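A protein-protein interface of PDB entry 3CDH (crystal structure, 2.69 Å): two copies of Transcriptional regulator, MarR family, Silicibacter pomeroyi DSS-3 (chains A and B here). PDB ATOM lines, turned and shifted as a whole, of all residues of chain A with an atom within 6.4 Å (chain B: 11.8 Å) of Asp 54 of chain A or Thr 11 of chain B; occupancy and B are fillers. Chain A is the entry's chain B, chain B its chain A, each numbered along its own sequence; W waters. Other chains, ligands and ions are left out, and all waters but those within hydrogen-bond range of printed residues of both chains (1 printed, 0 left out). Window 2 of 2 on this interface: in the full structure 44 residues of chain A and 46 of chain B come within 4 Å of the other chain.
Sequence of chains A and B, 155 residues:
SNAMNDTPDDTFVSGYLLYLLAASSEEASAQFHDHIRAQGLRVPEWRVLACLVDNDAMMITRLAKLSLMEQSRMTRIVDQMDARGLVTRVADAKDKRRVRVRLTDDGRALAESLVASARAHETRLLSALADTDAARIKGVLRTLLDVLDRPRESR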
ATOM      1  N   LEU A  49      -6.385  -1.583  11.503  1.00  0.00           N
ATOM      2  CA  LEU A  49      -7.723  -1.688  12.082  1.00  0.00           C
ATOM      3  C   LEU A  49      -8.146  -0.410  12.780  1.00  0.00           C
ATOM      4  O   LEU A  49      -9.278   0.068  12.595  1.00  0.00           O
ATOM      5  CB  LEU A  49      -7.827  -2.864  13.041  1.00  0.00           C
ATOM      6  CG  LEU A  49      -7.635  -4.246  12.425  1.00  0.00           C
ATOM      7  CD1 LEU A  49      -7.599  -5.228  13.553  1.00  0.00           C
ATOM      8  CD2 LEU A  49      -8.738  -4.614  11.435  1.00  0.00           C
ATOM      9  N   ALA A  50      -7.245   0.162  13.571  1.00  0.00           N
ATOM     10  CA  ALA A  50      -7.559   1.425  14.224  1.00  0.00           C
ATOM     11  C   ALA A  50      -7.922   2.517  13.189  1.00  0.00           C
ATOM     12  O   ALA A  50      -8.911   3.257  13.373  1.00  0.00           O
ATOM     13  CB  ALA A  50      -6.438   1.843  15.130  1.00  0.00           C
ATOM     14  N   CYS A  51      -7.175   2.593  12.086  1.00  0.00           N
ATOM     15  CA  CYS A  51      -7.491   3.604  11.059  1.00  0.00           C
ATOM     16  C   CYS A  51      -8.779   3.369  10.331  1.00  0.00           C
ATOM     17  O   CYS A  51      -9.357   4.314   9.826  1.00  0.00           O
ATOM     18  CB  CYS A  51      -6.428   3.683   9.984  1.00  0.00           C
ATOM     19  SG  CYS A  51      -4.889   4.170  10.600  1.00  0.00           S
ATOM     20  N   LEU A  52      -9.203   2.114  10.217  1.00  0.00           N
ATOM     21  CA  LEU A  52     -10.362   1.825   9.377  1.00  0.00           C
ATOM     22  C   LEU A  52     -11.668   1.744  10.142  1.00  0.00           C
ATOM     23  O   LEU A  52     -12.717   1.661   9.532  1.00  0.00           O
ATOM     24  CB  LEU A  52     -10.149   0.575   8.523  1.00  0.00           C
ATOM     25  CG  LEU A  52      -9.070   0.635   7.448  1.00  0.00           C
ATOM     26  CD1 LEU A  52      -8.998  -0.699   6.806  1.00  0.00           C
ATOM     27  CD2 LEU A  52      -9.364   1.671   6.403  1.00  0.00           C
ATOM     28  N   VAL A  53     -11.604   1.768  11.469  1.00  0.00           N
ATOM     29  CA  VAL A  53     -12.808   1.659  12.274  1.00  0.00           C
ATOM     30  C   VAL A  53     -13.823   2.781  11.989  1.00  0.00           C
ATOM     31  O   VAL A  53     -14.981   2.469  11.757  1.00  0.00           O
ATOM     32  CB  VAL A  53     -12.484   1.495  13.770  1.00  0.00           C
ATOM     33  CG1 VAL A  53     -12.219   2.829  14.429  1.00  0.00           C
ATOM     34  CG2 VAL A  53     -13.596   0.752  14.473  1.00  0.00           C
ATOM     35  N   ASP A  54     -13.406   4.056  11.966  1.00  0.00           N
ATOM     36  CA  ASP A  54     -14.347   5.144  11.617  1.00  0.00           C
ATOM     37  C   ASP A  54     -14.554   5.265  10.136  1.00  0.00           C
ATOM     38  O   ASP A  54     -15.683   5.345   9.695  1.00  0.00           O
ATOM     39  CB  ASP A  54     -13.916   6.534  12.057  1.00  0.00           C
ATOM     40  CG  ASP A  54     -13.236   6.542  13.364  1.00  0.00           C
ATOM     41  OD1 ASP A  54     -13.907   6.787  14.404  1.00  0.00           O
ATOM     42  OD2 ASP A  54     -12.017   6.305  13.330  1.00  0.00           O
ATOM     43  N   ASN A  55     -13.476   5.317   9.372  1.00  0.00           N
ATOM     44  CA  ASN A  55     -13.546   5.566   7.954  1.00  0.00           C
ATOM     45  C   ASN A  55     -14.128   4.385   7.175  1.00  0.00           C
ATOM     46  O   ASN A  55     -14.033   3.244   7.590  1.00  0.00           O
ATOM     47  CB  ASN A  55     -12.156   5.924   7.460  1.00  0.00           C
ATOM     48  CG  ASN A  55     -11.429   6.902   8.404  1.00  0.00           C
ATOM     49  OD1 ASN A  55     -11.025   6.547   9.527  1.00  0.00           O
ATOM     50  ND2 ASN A  55     -11.260   8.144   7.947  1.00  0.00           N
ATOM     51  N   ASP A  56     -14.765   4.658   6.049  1.00  0.00           N
ATOM     52  CA  ASP A  56     -15.327   3.578   5.247  1.00  0.00           C
ATOM     53  C   ASP A  56     -14.301   2.937   4.347  1.00  0.00           C
ATOM     54  O   ASP A  56     -14.399   1.757   4.059  1.00  0.00           O
ATOM     55  CB  ASP A  56     -16.470   4.086   4.374  1.00  0.00           C
ATOM     56  CG  ASP A  56     -17.797   4.100   5.103  1.00  0.00           C
ATOM     57  OD1 ASP A  56     -18.044   3.166   5.917  1.00  0.00           O
ATOM     58  OD2 ASP A  56     -18.592   5.041   4.846  1.00  0.00           O
ATOM     59  N   LEU A 103     -12.600  -2.387   5.828  1.00  0.00           N
ATOM     60  CA  LEU A 103     -12.828  -3.563   6.668  1.00  0.00           C
ATOM     61  C   LEU A 103     -13.906  -4.454   6.083  1.00  0.00           C
ATOM     62  O   LEU A 103     -14.852  -3.953   5.448  1.00  0.00           O
ATOM     63  CB  LEU A 103     -13.245  -3.150   8.068  1.00  0.00           C
ATOM     64  CG  LEU A 103     -12.133  -2.386   8.776  1.00  0.00           C
ATOM     65  CD1 LEU A 103     -12.580  -1.907  10.159  1.00  0.00           C
ATOM     66  CD2 LEU A 103     -10.865  -3.251   8.859  1.00  0.00           C
ATOM     67  N   ARG A 108     -14.391  -5.495  10.811  1.00  0.00           N
ATOM     68  CA  ARG A 108     -15.038  -4.427  11.544  1.00  0.00           C
ATOM     69  C   ARG A 108     -15.358  -4.862  12.971  1.00  0.00           C
ATOM     70  O   ARG A 108     -15.257  -4.068  13.913  1.00  0.00           O
ATOM     71  CB  ARG A 108     -16.274  -3.956  10.779  1.00  0.00           C
ATOM     72  CG  ARG A 108     -16.929  -2.677  11.279  1.00  0.00           C
ATOM     73  CD  ARG A 108     -17.877  -2.073  10.212  1.00  0.00           C
ATOM     74  NE  ARG A 108     -17.213  -1.226   9.195  1.00  0.00           N
ATOM     75  CZ  ARG A 108     -16.473  -0.131   9.460  1.00  0.00           C
ATOM     76  NH1 ARG A 108     -16.247   0.260  10.721  1.00  0.00           N
ATOM     77  NH2 ARG A 108     -15.922   0.577   8.462  1.00  0.00           N
ATOM     78  N   ARG A 119      -9.333   2.304  24.008  1.00  0.00           N
ATOM     79  CA  ARG A 119      -9.916   3.462  24.684  1.00  0.00           C
ATOM     80  C   ARG A 119      -9.856   3.319  26.199  1.00  0.00           C
ATOM     81  O   ARG A 119      -9.514   4.265  26.899  1.00  0.00           O
ATOM     82  CB  ARG A 119     -11.360   3.687  24.263  1.00  0.00           C
ATOM     83  CG  ARG A 119     -11.567   4.309  22.903  1.00  0.00           C
ATOM     84  CD  ARG A 119     -13.067   4.557  22.700  1.00  0.00           C
ATOM     85  NE  ARG A 119     -13.473   4.725  21.300  1.00  0.00           N
ATOM     86  CZ  ARG A 119     -13.395   5.875  20.618  1.00  0.00           C
ATOM     87  NH1 ARG A 119     -12.896   6.982  21.200  1.00  0.00           N
ATOM     88  NH2 ARG A 119     -13.811   5.916  19.342  1.00  0.00           N
ATOM     89  N   ASP B  10     -12.654  14.882  15.274  1.00  0.00           N
ATOM     90  CA  ASP B  10     -12.585  14.135  13.993  1.00  0.00           C
ATOM     91  C   ASP B  10     -12.754  12.595  14.183  1.00  0.00           C
ATOM     92  O   ASP B  10     -13.839  12.149  14.535  1.00  0.00           O
ATOM     93  CB  ASP B  10     -11.296  14.523  13.247  1.00  0.00           C
ATOM     94  CG  ASP B  10     -11.288  14.024  11.810  1.00  0.00           C
ATOM     95  OD1 ASP B  10     -10.251  13.445  11.379  1.00  0.00           O
ATOM     96  OD2 ASP B  10     -12.337  14.169  11.131  1.00  0.00           O
ATOM     97  N   THR B  11     -11.689  11.836  13.946  1.00  0.00           N
ATOM     98  CA  THR B  11     -11.756  10.381  14.013  1.00  0.00           C
ATOM     99  C   THR B  11     -11.094   9.857  15.283  1.00  0.00           C
ATOM    100  O   THR B  11     -10.599  10.631  16.102  1.00  0.00           O
ATOM    101  CB  THR B  11     -11.085   9.729  12.790  1.00  0.00           C
ATOM    102  OG1 THR B  11      -9.695  10.072  12.764  1.00  0.00           O
ATOM    103  CG2 THR B  11     -11.745  10.205  11.504  1.00  0.00           C
ATOM    104  N   PHE B  12     -11.091   8.537  15.440  1.00  0.00           N
ATOM    105  CA  PHE B  12     -10.529   7.909  16.630  1.00  0.00           C
ATOM    106  C   PHE B  12      -9.024   8.137  16.716  1.00  0.00           C
ATOM    107  O   PHE B  12      -8.528   8.715  17.682  1.00  0.00           O
ATOM    108  CB  PHE B  12     -10.835   6.410  16.640  1.00  0.00           C
ATOM    109  CG  PHE B  12      -9.931   5.612  17.535  1.00  0.00           C
ATOM    110  CD1 PHE B  12      -9.864   5.882  18.892  1.00  0.00           C
ATOM    111  CD2 PHE B  12      -9.148   4.592  17.021  1.00  0.00           C
ATOM    112  CE1 PHE B  12      -9.033   5.150  19.719  1.00  0.00           C
ATOM    113  CE2 PHE B  12      -8.316   3.856  17.842  1.00  0.00           C
ATOM    114  CZ  PHE B  12      -8.258   4.136  19.193  1.00  0.00           C
ATOM    115  N   VAL B  13      -8.302   7.677  15.699  1.00  0.00           N
ATOM    116  CA  VAL B  13      -6.856   7.862  15.640  1.00  0.00           C
ATOM    117  C   VAL B  13      -6.477   9.320  15.872  1.00  0.00           C
ATOM    118  O   VAL B  13      -5.444   9.615  16.472  1.00  0.00           O
ATOM    119  CB  VAL B  13      -6.284   7.402  14.286  1.00  0.00           C
ATOM    120  CG1 VAL B  13      -4.827   7.818  14.158  1.00  0.00           C
ATOM    121  CG2 VAL B  13      -6.430   5.896  14.133  1.00  0.00           C
ATOM    122  N   SER B  14      -7.320  10.230  15.393  1.00  0.00           N
ATOM    123  CA  SER B  14      -7.041  11.658  15.485  1.00  0.00           C
ATOM    124  C   SER B  14      -6.685  12.059  16.912  1.00  0.00           C
ATOM    125  O   SER B  14      -5.773  12.855  17.135  1.00  0.00           O
ATOM    126  CB  SER B  14      -8.240  12.471  14.993  1.00  0.00           C
ATOM    127  OG  SER B  14      -7.993  13.018  13.710  1.00  0.00           O
ATOM    128  N   GLY B  15      -7.412  11.503  17.877  1.00  0.00           N
ATOM    129  CA  GLY B  15      -7.345  11.971  19.248  1.00  0.00           C
ATOM    130  C   GLY B  15      -6.812  10.917  20.197  1.00  0.00           C
ATOM    131  O   GLY B  15      -6.836  11.094  21.415  1.00  0.00           O
ATOM    132  N   TYR B  16      -6.328   9.813  19.635  1.00  0.00           N
ATOM    133  CA  TYR B  16      -5.906   8.669  20.435  1.00  0.00           C
ATOM    134  C   TYR B  16      -4.467   8.827  20.906  1.00  0.00           C
ATOM    135  O   TYR B  16      -3.543   8.916  20.097  1.00  0.00           O
ATOM    136  CB  TYR B  16      -6.057   7.373  19.635  1.00  0.00           C
ATOM    137  CG  TYR B  16      -5.504   6.153  20.336  1.00  0.00           C
ATOM    138  CD1 TYR B  16      -5.823   5.884  21.660  1.00  0.00           C
ATOM    139  CD2 TYR B  16      -4.660   5.270  19.673  1.00  0.00           C
ATOM    140  CE1 TYR B  16      -5.320   4.771  22.305  1.00  0.00           C
ATOM    141  CE2 TYR B  16      -4.152   4.154  20.309  1.00  0.00           C
ATOM    142  CZ  TYR B  16      -4.484   3.909  21.626  1.00  0.00           C
ATOM    143  OH  TYR B  16      -3.980   2.799  22.262  1.00  0.00           O
ATOM    144  N   LEU B  17      -4.282   8.863  22.222  1.00  0.00           N
ATOM    145  CA  LEU B  17      -3.016   9.288  22.807  1.00  0.00           C
ATOM    146  C   LEU B  17      -1.809   8.539  22.248  1.00  0.00           C
ATOM    147  O   LEU B  17      -0.748   9.123  22.027  1.00  0.00           O
ATOM    148  CB  LEU B  17      -3.047   9.185  24.330  1.00  0.00           C
ATOM    149  CG  LEU B  17      -1.714   9.301  25.076  1.00  0.00           C
ATOM    150  CD1 LEU B  17      -1.219  10.694  25.006  1.00  0.00           C
ATOM    151  CD2 LEU B  17      -1.868   8.912  26.518  1.00  0.00           C
ATOM    152  N   LEU B  18      -1.949   7.249  22.013  1.00  0.00           N
ATOM    153  CA  LEU B  18      -0.796   6.505  21.537  1.00  0.00           C
ATOM    154  C   LEU B  18      -0.415   6.939  20.144  1.00  0.00           C
ATOM    155  O   LEU B  18       0.758   6.856  19.762  1.00  0.00           O
ATOM    156  CB  LEU B  18      -1.040   5.007  21.566  1.00  0.00           C
ATOM    157  CG  LEU B  18      -1.266   4.406  22.949  1.00  0.00           C
ATOM    158  CD1 LEU B  18      -1.177   2.888  22.817  1.00  0.00           C
ATOM    159  CD2 LEU B  18      -0.240   4.940  23.936  1.00  0.00           C
ATOM    160  N   TYR B  19      -1.392   7.409  19.373  1.00  0.00           N
ATOM    161  CA  TYR B  19      -1.056   7.858  18.034  1.00  0.00           C
ATOM    162  C   TYR B  19      -0.380   9.201  18.137  1.00  0.00           C
ATOM    163  O   TYR B  19       0.582   9.484  17.419  1.00  0.00           O
ATOM    164  CB  TYR B  19      -2.268   7.965  17.143  1.00  0.00           C
ATOM    165  CG  TYR B  19      -1.966   8.760  15.900  1.00  0.00           C
ATOM    166  CD1 TYR B  19      -2.256  10.124  15.838  1.00  0.00           C
ATOM    167  CD2 TYR B  19      -1.394   8.153  14.779  1.00  0.00           C
ATOM    168  CE1 TYR B  19      -1.985  10.860  14.711  1.00  0.00           C
ATOM    169  CE2 TYR B  19      -1.108   8.890  13.634  1.00  0.00           C
ATOM    170  CZ  TYR B  19      -1.410  10.240  13.621  1.00  0.00           C
ATOM    171  OH  TYR B  19      -1.147  10.980  12.509  1.00  0.00           O
ATOM    172  N   LEU B  20      -0.903  10.024  19.038  1.00  0.00           N
ATOM    173  CA  LEU B  20      -0.367  11.317  19.238  1.00  0.00           C
ATOM    174  C   LEU B  20       1.086  11.195  19.698  1.00  0.00           C
ATOM    175  O   LEU B  20       1.940  11.948  19.245  1.00  0.00           O
ATOM    176  CB  LEU B  20      -1.225  12.103  20.219  1.00  0.00           C
ATOM    177  CG  LEU B  20      -2.618  12.555  19.764  1.00  0.00           C
ATOM    178  CD1 LEU B  20      -3.345  13.166  20.933  1.00  0.00           C
ATOM    179  CD2 LEU B  20      -2.601  13.534  18.618  1.00  0.00           C
HETATM  180  O   HOH W   1      -9.454   6.144  13.259  1.00  0.00           O
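Of the printed residues of chain B, Ala 50 of chain A touches Phe 12 and Val 13. Printed residues of chain B within 4 Å of Cys 51 of chain A: Val 13. No residue of chain B comes within 4 Å of Asp 56 of chain A. Of the printed residues of chain B, Arg 119 of chain A touches Phe 12 (3.9 Å). Thr 11 of chain B touches just one residue of chain A: Asp 54 (3.6 Å). The nearest residue of chain B that does not touch Asp 54 of chain A is Val 13 of chain B (4.6 Å). The nearest printed residue of chain B that does not touch Arg 119 of chain A is Tyr 16 of chain B (5.0 Å).
The backbone NH (N) of Phe 12 of chain B lies within hydrogen-bond range of the side-chain carboxylate (OD2) of Asp 54 of chain A (3.2 Å).
Among the printed residues, pairs that only touch across the chains: Asp 54 of chain A with Thr 11 of chain B (3.6 Å), Ala 50 of chain A with Val 13 of chain B (3.7 Å), Ala 50 of chain A with Phe 12 of chain B (3.9 Å), Arg 119 of chain A with Phe 12 of chain B (3.9 Å) and Cys 51 of chain A with Val 13 of chain B (3.96 Å).
Water W1 lies within hydrogen-bond range of the side-chain carboxylate of Asp 54 of chain A, the backbone carbonyl oxygen of Ala 50 of chain A and the backbone NH of Val 13 of chain B.
O of Cys 51 of chain A sits close to OD1 of Asn 55 of chain A, at 2.8 Å.
Along chain B the printed residues that touch a printed residue of chain A span positions 11 to 13.
No position is printed for both chains. Of the 6 pairs that touch across the chains among the printed residues, none has its exchanged pair printed and touching as well.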
